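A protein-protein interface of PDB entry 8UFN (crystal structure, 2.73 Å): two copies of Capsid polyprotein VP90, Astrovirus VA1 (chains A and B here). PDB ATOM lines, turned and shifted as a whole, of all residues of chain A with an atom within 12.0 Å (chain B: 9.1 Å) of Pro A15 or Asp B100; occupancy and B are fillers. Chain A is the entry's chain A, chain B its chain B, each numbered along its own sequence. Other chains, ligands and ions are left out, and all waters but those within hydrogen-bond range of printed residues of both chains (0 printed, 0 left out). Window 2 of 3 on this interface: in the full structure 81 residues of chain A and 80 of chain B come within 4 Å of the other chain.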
ATOM      1  N   PRO A  15     -18.993  31.328  22.829  1.00  0.00           N
ATOM      2  CA  PRO A  15     -19.726  30.495  23.786  1.00  0.00           C
ATOM      3  C   PRO A  15     -21.089  31.087  24.139  1.00  0.00           C
ATOM      4  O   PRO A  15     -21.203  32.299  24.320  1.00  0.00           O
ATOM      5  CB  PRO A  15     -18.802  30.473  25.004  1.00  0.00           C
ATOM      6  CG  PRO A  15     -17.416  30.701  24.447  1.00  0.00           C
ATOM      7  CD  PRO A  15     -17.539  31.277  23.054  1.00  0.00           C
ATOM      8  N   ILE A  16     -22.102  30.238  24.232  1.00  0.00           N
ATOM      9  CA  ILE A  16     -23.483  30.666  24.449  1.00  0.00           C
ATOM     10  C   ILE A  16     -23.802  30.510  25.934  1.00  0.00           C
ATOM     11  O   ILE A  16     -23.643  29.406  26.471  1.00  0.00           O
ATOM     12  CB  ILE A  16     -24.471  29.850  23.594  1.00  0.00           C
ATOM     13  CG1 ILE A  16     -24.134  29.921  22.096  1.00  0.00           C
ATOM     14  CG2 ILE A  16     -25.895  30.334  23.825  1.00  0.00           C
ATOM     15  CD1 ILE A  16     -23.465  31.206  21.623  1.00  0.00           C
ATOM     16  N   PRO A  17     -24.255  31.557  26.615  1.00  0.00           N
ATOM     17  CA  PRO A  17     -24.489  31.471  28.057  1.00  0.00           C
ATOM     18  C   PRO A  17     -25.893  30.976  28.391  1.00  0.00           C
ATOM     19  O   PRO A  17     -26.793  30.945  27.550  1.00  0.00           O
ATOM     20  CB  PRO A  17     -24.295  32.922  28.528  1.00  0.00           C
ATOM     21  CG  PRO A  17     -24.432  33.784  27.283  1.00  0.00           C
ATOM     22  CD  PRO A  17     -24.585  32.888  26.083  1.00  0.00           C
ATOM     23  N   LEU A  18     -26.059  30.590  29.656  1.00  0.00           N
ATOM     24  CA  LEU A  18     -27.343  30.120  30.173  1.00  0.00           C
ATOM     25  C   LEU A  18     -28.199  31.339  30.487  1.00  0.00           C
ATOM     26  O   LEU A  18     -28.069  31.947  31.551  1.00  0.00           O
ATOM     27  CB  LEU A  18     -27.137  29.251  31.409  1.00  0.00           C
ATOM     28  CG  LEU A  18     -26.795  27.777  31.178  1.00  0.00           C
ATOM     29  CD1 LEU A  18     -26.094  27.190  32.394  1.00  0.00           C
ATOM     30  CD2 LEU A  18     -28.032  26.972  30.840  1.00  0.00           C
ATOM     31  N   THR A  19     -29.086  31.703  29.561  1.00  0.00           N
ATOM     32  CA  THR A  19     -29.856  32.937  29.654  1.00  0.00           C
ATOM     33  C   THR A  19     -31.339  32.636  29.489  1.00  0.00           C
ATOM     34  O   THR A  19     -31.732  31.920  28.563  1.00  0.00           O
ATOM     35  CB  THR A  19     -29.398  33.948  28.593  1.00  0.00           C
ATOM     36  OG1 THR A  19     -28.223  34.627  29.055  1.00  0.00           O
ATOM     37  CG2 THR A  19     -30.489  34.972  28.306  1.00  0.00           C
ATOM     38  N   TYR A  29     -31.027  18.222  31.374  1.00  0.00           N
ATOM     39  CA  TYR A  29     -29.966  17.241  31.527  1.00  0.00           C
ATOM     40  C   TYR A  29     -29.060  17.654  32.680  1.00  0.00           C
ATOM     41  O   TYR A  29     -28.682  18.823  32.793  1.00  0.00           O
ATOM     42  CB  TYR A  29     -29.142  17.101  30.249  1.00  0.00           C
ATOM     43  CG  TYR A  29     -27.879  16.309  30.464  1.00  0.00           C
ATOM     44  CD1 TYR A  29     -27.919  14.932  30.594  1.00  0.00           C
ATOM     45  CD2 TYR A  29     -26.651  16.945  30.585  1.00  0.00           C
ATOM     46  CE1 TYR A  29     -26.771  14.205  30.809  1.00  0.00           C
ATOM     47  CE2 TYR A  29     -25.500  16.227  30.806  1.00  0.00           C
ATOM     48  CZ  TYR A  29     -25.564  14.853  30.911  1.00  0.00           C
ATOM     49  OH  TYR A  29     -24.426  14.115  31.129  1.00  0.00           O
ATOM     50  N   SER A  92     -28.455  24.560  39.623  1.00  0.00           N
ATOM     51  CA  SER A  92     -27.154  24.906  39.068  1.00  0.00           C
ATOM     52  C   SER A  92     -26.478  23.746  38.352  1.00  0.00           C
ATOM     53  O   SER A  92     -25.643  23.979  37.469  1.00  0.00           O
ATOM     54  CB  SER A  92     -26.235  25.424  40.178  1.00  0.00           C
ATOM     55  OG  SER A  92     -26.019  24.426  41.162  1.00  0.00           O
ATOM     56  N   VAL A  94     -27.756  21.504  36.300  1.00  0.00           N
ATOM     57  CA  VAL A  94     -28.551  21.003  35.188  1.00  0.00           C
ATOM     58  C   VAL A  94     -28.411  21.934  33.994  1.00  0.00           C
ATOM     59  O   VAL A  94     -28.270  23.153  34.140  1.00  0.00           O
ATOM     60  CB  VAL A  94     -30.044  20.845  35.562  1.00  0.00           C
ATOM     61  CG1 VAL A  94     -30.260  19.577  36.371  1.00  0.00           C
ATOM     62  CG2 VAL A  94     -30.536  22.070  36.321  1.00  0.00           C
ATOM     63  N   LEU A  95     -28.447  21.344  32.803  1.00  0.00           N
ATOM     64  CA  LEU A  95     -28.585  22.086  31.560  1.00  0.00           C
ATOM     65  C   LEU A  95     -30.053  22.100  31.156  1.00  0.00           C
ATOM     66  O   LEU A  95     -30.750  21.090  31.290  1.00  0.00           O
ATOM     67  CB  LEU A  95     -27.747  21.465  30.441  1.00  0.00           C
ATOM     68  CG  LEU A  95     -26.281  21.143  30.731  1.00  0.00           C
ATOM     69  CD1 LEU A  95     -25.724  20.245  29.641  1.00  0.00           C
ATOM     70  CD2 LEU A  95     -25.459  22.419  30.851  1.00  0.00           C
ATOM     71  N   LEU A 104     -31.517  24.841  18.416  1.00  0.00           N
ATOM     72  CA  LEU A 104     -31.619  25.308  19.796  1.00  0.00           C
ATOM     73  C   LEU A 104     -32.432  26.595  19.845  1.00  0.00           C
ATOM     74  O   LEU A 104     -32.001  27.634  19.336  1.00  0.00           O
ATOM     75  CB  LEU A 104     -30.231  25.527  20.388  1.00  0.00           C
ATOM     76  CG  LEU A 104     -30.219  25.896  21.874  1.00  0.00           C
ATOM     77  CD1 LEU A 104     -29.957  24.668  22.728  1.00  0.00           C
ATOM     78  CD2 LEU A 104     -29.200  26.987  22.166  1.00  0.00           C
ATOM     79  N   GLY A 106     -33.319  27.906  22.830  1.00  0.00           N
ATOM     80  CA  GLY A 106     -32.843  28.619  23.998  1.00  0.00           C
ATOM     81  C   GLY A 106     -31.949  27.802  24.909  1.00  0.00           C
ATOM     82  O   GLY A 106     -32.213  26.624  25.165  1.00  0.00           O
ATOM     83  N   TRP A 107     -30.879  28.429  25.397  1.00  0.00           N
ATOM     84  CA  TRP A 107     -30.004  27.844  26.409  1.00  0.00           C
ATOM     85  C   TRP A 107     -30.355  28.517  27.734  1.00  0.00           C
ATOM     86  O   TRP A 107     -29.704  29.459  28.183  1.00  0.00           O
ATOM     87  CB  TRP A 107     -28.539  28.038  26.023  1.00  0.00           C
ATOM     88  CG  TRP A 107     -27.558  27.135  26.725  1.00  0.00           C
ATOM     89  CD1 TRP A 107     -26.517  27.521  27.519  1.00  0.00           C
ATOM     90  CD2 TRP A 107     -27.515  25.701  26.676  1.00  0.00           C
ATOM     91  NE1 TRP A 107     -25.834  26.421  27.974  1.00  0.00           N
ATOM     92  CE2 TRP A 107     -26.426  25.291  27.473  1.00  0.00           C
ATOM     93  CE3 TRP A 107     -28.290  24.727  26.045  1.00  0.00           C
ATOM     94  CZ2 TRP A 107     -26.094  23.951  27.654  1.00  0.00           C
ATOM     95  CZ3 TRP A 107     -27.960  23.394  26.225  1.00  0.00           C
ATOM     96  CH2 TRP A 107     -26.872  23.020  27.022  1.00  0.00           C
ATOM     97  N   ASN A 108     -31.421  28.024  28.356  1.00  0.00           N
ATOM     98  CA  ASN A 108     -32.078  28.696  29.468  1.00  0.00           C
ATOM     99  C   ASN A 108     -31.757  28.012  30.790  1.00  0.00           C
ATOM    100  O   ASN A 108     -31.113  26.963  30.838  1.00  0.00           O
ATOM    101  CB  ASN A 108     -33.595  28.731  29.246  1.00  0.00           C
ATOM    102  CG  ASN A 108     -33.970  29.236  27.868  1.00  0.00           C
ATOM    103  OD1 ASN A 108     -34.693  28.571  27.127  1.00  0.00           O
ATOM    104  ND2 ASN A 108     -33.479  30.420  27.516  1.00  0.00           N
ATOM    105  N   ILE B  16     -30.374  28.019  16.423  1.00  0.00           N
ATOM    106  CA  ILE B  16     -29.003  27.659  16.072  1.00  0.00           C
ATOM    107  C   ILE B  16     -29.044  26.316  15.350  1.00  0.00           C
ATOM    108  O   ILE B  16     -29.344  25.290  15.986  1.00  0.00           O
ATOM    109  CB  ILE B  16     -28.101  27.598  17.310  1.00  0.00           C
ATOM    110  CG1 ILE B  16     -28.447  28.733  18.277  1.00  0.00           C
ATOM    111  CG2 ILE B  16     -26.637  27.667  16.905  1.00  0.00           C
ATOM    112  CD1 ILE B  16     -27.547  28.796  19.488  1.00  0.00           C
ATOM    113  N   VAL B  23     -15.908  19.452  18.567  1.00  0.00           N
ATOM    114  CA  VAL B  23     -14.490  19.637  18.850  1.00  0.00           C
ATOM    115  C   VAL B  23     -14.282  19.421  20.344  1.00  0.00           C
ATOM    116  O   VAL B  23     -14.820  20.171  21.167  1.00  0.00           O
ATOM    117  CB  VAL B  23     -14.001  21.029  18.419  1.00  0.00           C
ATOM    118  CG1 VAL B  23     -12.496  21.143  18.597  1.00  0.00           C
ATOM    119  CG2 VAL B  23     -14.399  21.307  16.976  1.00  0.00           C
ATOM    120  N   ASP B  25     -14.484  16.974  23.886  1.00  0.00           N
ATOM    121  CA  ASP B  25     -15.516  16.140  24.485  1.00  0.00           C
ATOM    122  C   ASP B  25     -16.896  16.704  24.175  1.00  0.00           C
ATOM    123  O   ASP B  25     -17.108  17.920  24.195  1.00  0.00           O
ATOM    124  CB  ASP B  25     -15.312  16.033  25.996  1.00  0.00           C
ATOM    125  CG  ASP B  25     -15.184  17.388  26.666  1.00  0.00           C
ATOM    126  OD1 ASP B  25     -14.921  18.382  25.959  1.00  0.00           O
ATOM    127  OD2 ASP B  25     -15.343  17.456  27.903  1.00  0.00           O
ATOM    128  N   TYR B  27     -21.440  15.791  23.986  1.00  0.00           N
ATOM    129  CA  TYR B  27     -22.602  15.025  24.400  1.00  0.00           C
ATOM    130  C   TYR B  27     -23.388  14.550  23.185  1.00  0.00           C
ATOM    131  O   TYR B  27     -23.454  15.233  22.161  1.00  0.00           O
ATOM    132  CB  TYR B  27     -23.527  15.852  25.290  1.00  0.00           C
ATOM    133  CG  TYR B  27     -23.002  16.163  26.670  1.00  0.00           C
ATOM    134  CD1 TYR B  27     -22.231  17.294  26.914  1.00  0.00           C
ATOM    135  CD2 TYR B  27     -23.349  15.363  27.746  1.00  0.00           C
ATOM    136  CE1 TYR B  27     -21.783  17.585  28.191  1.00  0.00           C
ATOM    137  CE2 TYR B  27     -22.897  15.636  29.010  1.00  0.00           C
ATOM    138  CZ  TYR B  27     -22.124  16.749  29.236  1.00  0.00           C
ATOM    139  OH  TYR B  27     -21.687  17.012  30.515  1.00  0.00           O
ATOM    140  N   TRP B  97     -23.856  18.227  21.194  1.00  0.00           N
ATOM    141  CA  TRP B  97     -23.422  19.519  21.699  1.00  0.00           C
ATOM    142  C   TRP B  97     -22.174  19.342  22.548  1.00  0.00           C
ATOM    143  O   TRP B  97     -21.979  18.307  23.192  1.00  0.00           O
ATOM    144  CB  TRP B  97     -24.524  20.217  22.511  1.00  0.00           C
ATOM    145  CG  TRP B  97     -24.791  19.618  23.860  1.00  0.00           C
ATOM    146  CD1 TRP B  97     -24.178  19.934  25.037  1.00  0.00           C
ATOM    147  CD2 TRP B  97     -25.762  18.613  24.173  1.00  0.00           C
ATOM    148  NE1 TRP B  97     -24.699  19.181  26.060  1.00  0.00           N
ATOM    149  CE2 TRP B  97     -25.676  18.364  25.556  1.00  0.00           C
ATOM    150  CE3 TRP B  97     -26.693  17.897  23.415  1.00  0.00           C
ATOM    151  CZ2 TRP B  97     -26.483  17.427  26.198  1.00  0.00           C
ATOM    152  CZ3 TRP B  97     -27.494  16.971  24.052  1.00  0.00           C
ATOM    153  CH2 TRP B  97     -27.383  16.743  25.430  1.00  0.00           C
ATOM    154  N   THR B  98     -21.324  20.363  22.531  1.00  0.00           N
ATOM    155  CA  THR B  98     -20.122  20.411  23.349  1.00  0.00           C
ATOM    156  C   THR B  98     -20.158  21.671  24.206  1.00  0.00           C
ATOM    157  O   THR B  98     -20.743  22.689  23.821  1.00  0.00           O
ATOM    158  CB  THR B  98     -18.854  20.351  22.475  1.00  0.00           C
ATOM    159  OG1 THR B  98     -17.762  19.818  23.237  1.00  0.00           O
ATOM    160  CG2 THR B  98     -18.483  21.717  21.924  1.00  0.00           C
ATOM    161  N   LEU B  99     -19.551  21.588  25.388  1.00  0.00           N
ATOM    162  CA  LEU B  99     -19.764  22.571  26.438  1.00  0.00           C
ATOM    163  C   LEU B  99     -18.476  23.297  26.806  1.00  0.00           C
ATOM    164  O   LEU B  99     -17.377  22.741  26.722  1.00  0.00           O
ATOM    165  CB  LEU B  99     -20.342  21.912  27.698  1.00  0.00           C
ATOM    166  CG  LEU B  99     -21.830  21.561  27.679  1.00  0.00           C
ATOM    167  CD1 LEU B  99     -22.223  20.892  28.984  1.00  0.00           C
ATOM    168  CD2 LEU B  99     -22.675  22.802  27.433  1.00  0.00           C
ATOM    169  N   ASP B 100     -18.636  24.551  27.220  1.00  0.00           N
ATOM    170  CA  ASP B 100     -17.572  25.364  27.803  1.00  0.00           C
ATOM    171  C   ASP B 100     -17.916  25.536  29.280  1.00  0.00           C
ATOM    172  O   ASP B 100     -18.493  26.540  29.695  1.00  0.00           O
ATOM    173  CB  ASP B 100     -17.450  26.714  27.075  1.00  0.00           C
ATOM    174  CG  ASP B 100     -16.310  27.566  27.603  1.00  0.00           C
ATOM    175  OD1 ASP B 100     -15.482  27.049  28.382  1.00  0.00           O
ATOM    176  OD2 ASP B 100     -16.246  28.759  27.239  1.00  0.00           O
ATOM    177  N   GLY B 101     -17.558  24.533  30.079  1.00  0.00           N
ATOM    178  CA  GLY B 101     -18.015  24.481  31.453  1.00  0.00           C
ATOM    179  C   GLY B 101     -19.470  24.064  31.513  1.00  0.00           C
ATOM    180  O   GLY B 101     -19.782  22.870  31.541  1.00  0.00           O
ATOM    181  N   GLN B 102     -20.374  25.046  31.528  1.00  0.00           N
ATOM    182  CA  GLN B 102     -21.800  24.790  31.369  1.00  0.00           C
ATOM    183  C   GLN B 102     -22.417  25.681  30.300  1.00  0.00           C
ATOM    184  O   GLN B 102     -23.646  25.717  30.173  1.00  0.00           O
ATOM    185  CB  GLN B 102     -22.543  24.969  32.700  1.00  0.00           C
ATOM    186  CG  GLN B 102     -22.358  23.808  33.666  1.00  0.00           C
ATOM    187  CD  GLN B 102     -23.669  23.317  34.252  1.00  0.00           C
ATOM    188  OE1 GLN B 102     -24.631  24.075  34.374  1.00  0.00           O
ATOM    189  NE2 GLN B 102     -23.712  22.040  34.616  1.00  0.00           N
ATOM    190  N   LYS B 103     -21.600  26.398  29.534  1.00  0.00           N
ATOM    191  CA  LYS B 103     -22.064  27.225  28.431  1.00  0.00           C
ATOM    192  C   LYS B 103     -21.941  26.461  27.119  1.00  0.00           C
ATOM    193  O   LYS B 103     -21.026  25.657  26.929  1.00  0.00           O
ATOM    194  CB  LYS B 103     -21.269  28.533  28.354  1.00  0.00           C
ATOM    195  CG  LYS B 103     -20.729  29.016  29.693  1.00  0.00           C
ATOM    196  CD  LYS B 103     -19.298  29.523  29.570  1.00  0.00           C
ATOM    197  CE  LYS B 103     -18.654  29.678  30.941  1.00  0.00           C
ATOM    198  NZ  LYS B 103     -17.168  29.751  30.859  1.00  0.00           N
ATOM    199  N   LEU B 104     -22.880  26.717  26.211  1.00  0.00           N
ATOM    200  CA  LEU B 104     -22.898  26.025  24.929  1.00  0.00           C
ATOM    201  C   LEU B 104     -21.798  26.567  24.026  1.00  0.00           C
ATOM    202  O   LEU B 104     -21.797  27.752  23.676  1.00  0.00           O
ATOM    203  CB  LEU B 104     -24.260  26.179  24.261  1.00  0.00           C
ATOM    204  CG  LEU B 104     -24.549  25.199  23.122  1.00  0.00           C
ATOM    205  CD1 LEU B 104     -24.288  23.767  23.566  1.00  0.00           C
ATOM    206  CD2 LEU B 104     -25.975  25.361  22.625  1.00  0.00           C
ATOM    207  N   SER B 105     -20.863  25.699  23.648  1.00  0.00           N
ATOM    208  CA  SER B 105     -19.793  26.057  22.729  1.00  0.00           C
ATOM    209  C   SER B 105     -19.940  25.396  21.365  1.00  0.00           C
ATOM    210  O   SER B 105     -19.084  25.601  20.498  1.00  0.00           O
ATOM    211  CB  SER B 105     -18.432  25.708  23.342  1.00  0.00           C
ATOM    212  OG  SER B 105     -18.321  24.320  23.593  1.00  0.00           O
ATOM    213  N   GLY B 106     -21.002  24.624  21.146  1.00  0.00           N
ATOM    214  CA  GLY B 106     -21.219  23.997  19.857  1.00  0.00           C
ATOM    215  C   GLY B 106     -22.511  23.210  19.756  1.00  0.00           C
ATOM    216  O   GLY B 106     -22.824  22.401  20.633  1.00  0.00           O
ATOM    217  N   HIS B 283     -22.040  11.122  27.133  1.00  0.00           N
ATOM    218  CA  HIS B 283     -20.904  12.025  27.013  1.00  0.00           C
ATOM    219  C   HIS B 283     -19.689  11.243  26.536  1.00  0.00           C
ATOM    220  O   HIS B 283     -19.382  10.172  27.073  1.00  0.00           O
ATOM    221  CB  HIS B 283     -20.602  12.723  28.340  1.00  0.00           C
ATOM    222  CG  HIS B 283     -19.636  13.858  28.212  1.00  0.00           C
ATOM    223  ND1 HIS B 283     -20.011  15.107  27.769  1.00  0.00           N
ATOM    224  CD2 HIS B 283     -18.308  13.932  28.467  1.00  0.00           C
ATOM    225  CE1 HIS B 283     -18.958  15.902  27.756  1.00  0.00           C
ATOM    226  NE2 HIS B 283     -17.911  15.215  28.175  1.00  0.00           N
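Among the printed residues, merely in contact across the chains: Tyr A29 with Tyr B27 (3.0 Å), Ile A16 with Lys B103 (3.2 Å), Pro A15 with Leu B104 (3.4 Å), Pro A15 with Asp B100 (3.6 Å), Trp A107 with Leu B99 (3.6 Å), Leu A18 with Gln B102 (3.6 Å), Leu A95 with Leu B99 (3.6 Å), Leu A104 with Leu B104 (3.6 Å), Val A94 with Gln B102 (3.8 Å), Leu A95 with Gln B102 (3.8 Å), Leu A95 with Trp B97 (3.9 Å) and Trp A107 with Lys B103 (3.9 Å).
Printed residues of chain B that touch a printed residue of chain A: Ile B16, Tyr B27, Trp B97, Leu B99, Asp B100, Gln B102, Lys B103 and Leu B104. Hydrophobic or aromatic side chains of chain B within 4 Å of the printed part of chain A: Ile B16, Tyr B27, Trp B97, Leu B99 and Leu B104. Hydrophobic or aromatic side chains of chain A that line the printed part of chain B: Pro A15, Ile A16, Leu A18, Tyr A29, Leu A95, Leu A104 and Trp A107. Among the printed residues, 17 pairs touch across the chains. Among the printed residues, no Asp or Glu carboxylate lies within 4 Å of a Lys or Arg side-chain nitrogen of the other chain.
The backbone NH (N) of Thr A19 sits at hydrogen-bond distance from the backbone carbonyl oxygen (O) of Trp A107 (2.7 Å). N of Leu A95 lies within hydrogen-bond range of O of Tyr A29 (2.5 Å). The backbone NH (N) of Tyr B27 lies within hydrogen-bond range of the backbone carbonyl oxygen (O) of Trp B97 (2.7 Å). N of Leu B99 sits close to OG of Ser B105, 3.5 Å away. NZ of Lys B103 is in salt-bridge range of OD2 of Asp B100 (3.9 Å).
Of chain B, only Asp B100 and Leu B104 come within 4 Å of Pro A15. Printed residues of chain A within 4 Å of Asp B100: Pro A15 (3.6 Å). Of chain B, only Lys B103 (3.2 Å) and Leu B104 (2.6 Å) come within 4 Å of Ile A16. No residue of chain A comes within 4 Å of Thr B98. Leu B99 touches just these residues of chain A: Leu A95 and Trp A107. No residue of chain A comes within 4 Å of Gly B101. Lys B103 touches two residues of chain A. Leu B104 touches just these residues of chain A: Pro A15 (3.4 Å), Ile A16 (2.6 Å), Leu A104 (3.6 Å) and Trp A107 (3.5 Å). No residue of chain A comes within 4 Å of Ser B105. Of the printed residues of chain B, Ser A92 touches Gln B102 (3.3 Å). Printed residues of chain A within 4 Å of Ile B16: Leu A104 (3.3 Å). Of the printed residues of chain A, Trp B97 touches Leu A95 (3.9 Å). The nearest printed residue of chain B that does not touch Pro A15 is Ser B105 (4.6 Å).
The backbone carbonyl oxygen (O) of Leu B104 is in hydrogen-bond range of the backbone NH (N) of Ile A16 (2.6 Å). The backbone carbonyl oxygen (O) of Ser A92 lies close to the side-chain amide oxygen (OE1) of Gln B102, at 3.3 Å. The backbone NH of Leu A104 lies within hydrogen-bond range of the backbone carbonyl oxygen of Ile B16, 3.3 Å away. NE1 of Trp A107 is in hydrogen-bond range of O of Gln B102 (3.2 Å). The backbone NH of Leu B104 lies close to the indole nitrogen of Trp A107 (3.5 Å).
Ile A16 touches Leu B104, and with the chains exchanged Leu A104 touches Ile B16. Leu A104 touches its own counterpart, Leu B104. Of the 17 pairs that touch across the chains among the printed residues, 3 have their exchanged pair printed and touching as well.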
